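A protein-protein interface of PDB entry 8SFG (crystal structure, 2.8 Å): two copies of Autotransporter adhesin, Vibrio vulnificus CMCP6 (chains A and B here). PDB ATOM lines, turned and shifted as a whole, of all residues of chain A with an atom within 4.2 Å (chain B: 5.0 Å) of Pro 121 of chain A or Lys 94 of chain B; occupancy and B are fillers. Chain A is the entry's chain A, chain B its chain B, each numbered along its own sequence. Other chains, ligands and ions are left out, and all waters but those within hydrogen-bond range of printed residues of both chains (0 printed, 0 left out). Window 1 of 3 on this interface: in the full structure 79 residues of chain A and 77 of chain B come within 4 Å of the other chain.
The backbone carbonyl oxygen (O) of Pro 121 of chain A lies within hydrogen-bond range of the side-chain amino group (NZ) of Lys 94 of chain B. The backbone carbonyl oxygen of Gln 122 of chain A is in hydrogen-bond range of the backbone NH of Lys 94 of chain B (2.9 Å). The backbone NH of Met 124 of chain A sits at hydrogen-bond distance from the backbone carbonyl oxygen of Gln 92 of chain B (2.8 Å). The backbone carbonyl oxygen (O) of Ala 271 of chain A is in hydrogen-bond range of the side-chain amino group (NZ) of Lys 94 of chain B (2.9 Å).
NE2 of Gln 122 of chain A lies within hydrogen-bond range of O of Gln 118 of chain A, 3.0 Å away.
Among the printed residues, merely in contact across the chains: Gln 122 of chain A with Asn 93 of chain B (3.7 Å), Leu 123 of chain A with Gln 92 of chain B (3.2 Å), Leu 123 of chain A with Asn 93 of chain B (3.7 Å), Leu 123 of chain A with Lys 94 of chain B (3.1 Å), Met 124 of chain A with Asn 93 of chain B (3.97 Å), Met 124 of chain A with Lys 94 of chain B (3.4 Å), Met 124 of chain A with Ser 95 of chain B (3.0 Å), Asn 270 of chain A with Lys 94 of chain B (3.98 Å) and Gly 272 of chain A with Lys 94 of chain B (3.8 Å).
Of chain B, only Lys 94 comes within 4 Å of Pro 121 of chain A. Of chain A, only Pro 121 (3.0 Å), Gln 122 (2.9 Å), Leu 123 (3.1 Å), Met 124 (3.4 Å), Asn 270 (3.98 Å), Ala 271 (2.9 Å) and Gly 272 (3.8 Å) come within 4 Å of Lys 94 of chain B. Of the printed residues of chain B, Ala 271 of chain A touches Lys 94. Of the printed residues of chain A, Gln 92 of chain B touches Leu 123 and Met 124. Printed residues of chain B within 4 Å of Asn 270 of chain A: Lys 94. Of the printed residues of chain B, Gln 122 of chain A touches Asn 93 and Lys 94. Printed residues of chain B within 4 Å of Leu 123 of chain A: Gln 92, Asn 93 and Lys 94. Leu 119 of chain A touches none of the printed residues of chain B. Glu 96 of chain B touches none of the printed residues of chain A. The nearest printed residue of chain B that does not touch Pro 121 of chain A is Asn 99 of chain B (5.8 Å).
Along chain B the printed residues that touch a printed residue of chain A span positions 92 to 95. Hydrophobic or aromatic side chains of chain A within 4 Å of the printed part of chain B: Leu 123 and Met 124.
No position is printed for both chains.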
ATOM      1  N   GLU A 117       3.119 -23.097  19.710  1.00  0.00           N
ATOM      2  CA  GLU A 117       4.008 -23.205  20.900  1.00  0.00           C
ATOM      3  C   GLU A 117       4.331 -21.811  21.434  1.00  0.00           C
ATOM      4  O   GLU A 117       4.359 -21.655  22.652  1.00  0.00           O
ATOM      5  CB  GLU A 117       5.292 -23.951  20.540  1.00  0.00           C
ATOM      6  CG  GLU A 117       6.304 -24.055  21.663  1.00  0.00           C
ATOM      7  CD  GLU A 117       7.473 -24.977  21.364  1.00  0.00           C
ATOM      8  OE1 GLU A 117       7.480 -25.598  20.277  1.00  0.00           O
ATOM      9  OE2 GLU A 117       8.378 -25.074  22.213  1.00  0.00           O
ATOM     10  N   GLN A 118       4.558 -20.852  20.538  1.00  0.00           N
ATOM     11  CA  GLN A 118       4.911 -19.447  20.884  1.00  0.00           C
ATOM     12  C   GLN A 118       3.649 -18.628  21.182  1.00  0.00           C
ATOM     13  O   GLN A 118       3.747 -17.661  21.968  1.00  0.00           O
ATOM     14  CB  GLN A 118       5.644 -18.819  19.695  1.00  0.00           C
ATOM     15  CG  GLN A 118       6.731 -19.719  19.121  1.00  0.00           C
ATOM     16  CD  GLN A 118       7.314 -19.193  17.832  1.00  0.00           C
ATOM     17  OE1 GLN A 118       7.755 -18.050  17.747  1.00  0.00           O
ATOM     18  NE2 GLN A 118       7.334 -20.046  16.816  1.00  0.00           N
ATOM     19  N   LEU A 119       2.512 -19.009  20.586  1.00  0.00           N
ATOM     20  CA  LEU A 119       1.228 -18.264  20.745  1.00  0.00           C
ATOM     21  C   LEU A 119       0.471 -18.638  22.035  1.00  0.00           C
ATOM     22  O   LEU A 119       0.000 -17.723  22.721  1.00  0.00           O
ATOM     23  CB  LEU A 119       0.370 -18.553  19.509  1.00  0.00           C
ATOM     24  CG  LEU A 119      -0.987 -17.853  19.452  1.00  0.00           C
ATOM     25  CD1 LEU A 119      -0.820 -16.334  19.434  1.00  0.00           C
ATOM     26  CD2 LEU A 119      -1.769 -18.310  18.220  1.00  0.00           C
ATOM     27  N   ALA A 120       0.347 -19.932  22.339  1.00  0.00           N
ATOM     28  CA  ALA A 120      -0.402 -20.438  23.519  1.00  0.00           C
ATOM     29  C   ALA A 120      -0.064 -19.678  24.799  1.00  0.00           C
ATOM     30  O   ALA A 120      -0.972 -19.287  25.521  1.00  0.00           O
ATOM     31  CB  ALA A 120      -0.159 -21.918  23.693  1.00  0.00           C
ATOM     32  N   PRO A 121       1.226 -19.464  25.152  1.00  0.00           N
ATOM     33  CA  PRO A 121       1.582 -18.750  26.383  1.00  0.00           C
ATOM     34  C   PRO A 121       1.129 -17.286  26.471  1.00  0.00           C
ATOM     35  O   PRO A 121       1.175 -16.742  27.554  1.00  0.00           O
ATOM     36  CB  PRO A 121       3.120 -18.761  26.395  1.00  0.00           C
ATOM     37  CG  PRO A 121       3.490 -19.915  25.490  1.00  0.00           C
ATOM     38  CD  PRO A 121       2.412 -19.928  24.423  1.00  0.00           C
ATOM     39  N   GLN A 122       0.704 -16.699  25.349  1.00  0.00           N
ATOM     40  CA  GLN A 122       0.265 -15.276  25.302  1.00  0.00           C
ATOM     41  C   GLN A 122      -1.263 -15.188  25.408  1.00  0.00           C
ATOM     42  O   GLN A 122      -1.770 -14.069  25.565  1.00  0.00           O
ATOM     43  CB  GLN A 122       0.676 -14.630  23.974  1.00  0.00           C
ATOM     44  CG  GLN A 122       2.162 -14.728  23.631  1.00  0.00           C
ATOM     45  CD  GLN A 122       2.468 -14.215  22.241  1.00  0.00           C
ATOM     46  OE1 GLN A 122       1.727 -13.408  21.666  1.00  0.00           O
ATOM     47  NE2 GLN A 122       3.587 -14.664  21.691  1.00  0.00           N
ATOM     48  N   LEU A 123      -1.967 -16.323  25.356  1.00  0.00           N
ATOM     49  CA  LEU A 123      -3.456 -16.316  25.388  1.00  0.00           C
ATOM     50  C   LEU A 123      -4.003 -16.678  26.768  1.00  0.00           C
ATOM     51  O   LEU A 123      -3.286 -17.174  27.636  1.00  0.00           O
ATOM     52  CB  LEU A 123      -3.966 -17.303  24.330  1.00  0.00           C
ATOM     53  CG  LEU A 123      -3.490 -17.044  22.897  1.00  0.00           C
ATOM     54  CD1 LEU A 123      -3.994 -18.114  21.941  1.00  0.00           C
ATOM     55  CD2 LEU A 123      -3.923 -15.667  22.418  1.00  0.00           C
ATOM     56  N   MET A 124      -5.305 -16.402  26.938  1.00  0.00           N
ATOM     57  CA  MET A 124      -6.056 -16.685  28.152  1.00  0.00           C
ATOM     58  C   MET A 124      -7.313 -17.435  27.718  1.00  0.00           C
ATOM     59  O   MET A 124      -7.719 -17.305  26.567  1.00  0.00           O
ATOM     60  CB  MET A 124      -6.382 -15.381  28.885  1.00  0.00           C
ATOM     61  CG  MET A 124      -7.573 -14.629  28.317  1.00  0.00           C
ATOM     62  SD  MET A 124      -8.168 -13.175  29.490  1.00  0.00           S
ATOM     63  CE  MET A 124      -6.638 -12.064  29.991  1.00  0.00           C
ATOM     64  N   ASN A 270      -7.156 -16.544  33.588  1.00  0.00           N
ATOM     65  CA  ASN A 270      -6.847 -15.148  33.171  1.00  0.00           C
ATOM     66  C   ASN A 270      -5.332 -14.943  33.027  1.00  0.00           C
ATOM     67  O   ASN A 270      -4.900 -14.474  31.967  1.00  0.00           O
ATOM     68  CB  ASN A 270      -7.435 -14.130  34.156  1.00  0.00           C
ATOM     69  CG  ASN A 270      -8.953 -14.114  34.169  1.00  0.00           C
ATOM     70  OD1 ASN A 270      -9.588 -14.402  33.153  1.00  0.00           O
ATOM     71  ND2 ASN A 270      -9.542 -13.753  35.302  1.00  0.00           N
ATOM     72  N   ALA A 271      -4.558 -15.282  34.055  1.00  0.00           N
ATOM     73  CA  ALA A 271      -3.090 -15.086  34.012  1.00  0.00           C
ATOM     74  C   ALA A 271      -2.381 -16.230  33.279  1.00  0.00           C
ATOM     75  O   ALA A 271      -1.219 -16.027  32.870  1.00  0.00           O
ATOM     76  CB  ALA A 271      -2.578 -14.972  35.423  1.00  0.00           C
ATOM     77  N   GLY A 272      -3.041 -17.379  33.114  1.00  0.00           N
ATOM     78  CA  GLY A 272      -2.374 -18.523  32.468  1.00  0.00           C
ATOM     79  C   GLY A 272      -1.437 -19.201  33.452  1.00  0.00           C
ATOM     80  O   GLY A 272      -1.658 -19.041  34.672  1.00  0.00           O
ATOM     81  N   GLN B  92      -8.005 -15.498  23.845  1.00  0.00           N
ATOM     82  CA  GLN B  92      -7.853 -14.044  23.608  1.00  0.00           C
ATOM     83  C   GLN B  92      -6.514 -13.634  24.210  1.00  0.00           C
ATOM     84  O   GLN B  92      -6.022 -14.365  25.087  1.00  0.00           O
ATOM     85  CB  GLN B  92      -9.043 -13.301  24.219  1.00  0.00           C
ATOM     86  CG  GLN B  92      -9.011 -11.795  24.002  1.00  0.00           C
ATOM     87  CD  GLN B  92     -10.216 -11.104  24.588  1.00  0.00           C
ATOM     88  OE1 GLN B  92     -10.998 -11.686  25.339  1.00  0.00           O
ATOM     89  NE2 GLN B  92     -10.370  -9.834  24.253  1.00  0.00           N
ATOM     90  N   ASN B  93      -5.934 -12.534  23.730  1.00  0.00           N
ATOM     91  CA  ASN B  93      -4.635 -12.048  24.260  1.00  0.00           C
ATOM     92  C   ASN B  93      -4.781 -11.802  25.763  1.00  0.00           C
ATOM     93  O   ASN B  93      -5.860 -11.330  26.163  1.00  0.00           O
ATOM     94  CB  ASN B  93      -4.204 -10.779  23.532  1.00  0.00           C
ATOM     95  CG  ASN B  93      -4.171 -10.961  22.032  1.00  0.00           C
ATOM     96  OD1 ASN B  93      -4.199 -12.084  21.530  1.00  0.00           O
ATOM     97  ND2 ASN B  93      -4.113  -9.861  21.304  1.00  0.00           N
ATOM     98  N   LYS B  94      -3.754 -12.133  26.556  1.00  0.00           N
ATOM     99  CA  LYS B  94      -3.815 -11.906  28.022  1.00  0.00           C
ATOM    100  C   LYS B  94      -3.817 -10.407  28.299  1.00  0.00           C
ATOM    101  O   LYS B  94      -3.115  -9.687  27.561  1.00  0.00           O
ATOM    102  CB  LYS B  94      -2.606 -12.482  28.768  1.00  0.00           C
ATOM    103  CG  LYS B  94      -2.512 -13.997  28.821  1.00  0.00           C
ATOM    104  CD  LYS B  94      -1.286 -14.485  29.559  1.00  0.00           C
ATOM    105  CE  LYS B  94      -1.202 -15.996  29.618  1.00  0.00           C
ATOM    106  NZ  LYS B  94       0.023 -16.451  30.314  1.00  0.00           N
ATOM    107  N   SER B  95      -4.543  -9.984  29.346  1.00  0.00           N
ATOM    108  CA  SER B  95      -4.605  -8.546  29.718  1.00  0.00           C
ATOM    109  C   SER B  95      -3.190  -8.087  30.068  1.00  0.00           C
ATOM    110  O   SER B  95      -2.433  -8.908  30.606  1.00  0.00           O
ATOM    111  CB  SER B  95      -5.564  -8.319  30.845  1.00  0.00           C
ATOM    112  OG  SER B  95      -6.860  -8.763  30.485  1.00  0.00           O
ATOM    113  N   GLU B  96      -2.864  -6.829  29.773  1.00  0.00           N
ATOM    114  CA  GLU B  96      -1.506  -6.281  30.003  1.00  0.00           C
ATOM    115  C   GLU B  96      -1.130  -6.311  31.491  1.00  0.00           C
ATOM    116  O   GLU B  96       0.064  -6.508  31.769  1.00  0.00           O
ATOM    117  CB  GLU B  96      -1.446  -4.866  29.418  1.00  0.00           C
ATOM    118  CG  GLU B  96      -0.158  -4.117  29.708  1.00  0.00           C
ATOM    119  CD  GLU B  96       1.126  -4.728  29.171  1.00  0.00           C
ATOM    120  OE1 GLU B  96       1.084  -5.837  28.576  1.00  0.00           O
ATOM    121  OE2 GLU B  96       2.179  -4.059  29.314  1.00  0.00           O
ATOM    122  N   ASN B  99       0.750  -9.507  32.448  1.00  0.00           N
ATOM    123  CA  ASN B  99       2.124  -9.523  31.878  1.00  0.00           C
ATOM    124  C   ASN B  99       2.993  -8.526  32.651  1.00  0.00           C
ATOM    125  O   ASN B  99       4.174  -8.840  32.899  1.00  0.00           O
ATOM    126  CB  ASN B  99       2.120  -9.214  30.379  1.00  0.00           C
ATOM    127  CG  ASN B  99       1.493 -10.309  29.542  1.00  0.00           C
ATOM    128  OD1 ASN B  99       1.596 -11.490  29.866  1.00  0.00           O
ATOM    129  ND2 ASN B  99       0.878  -9.931  28.437  1.00  0.00           N
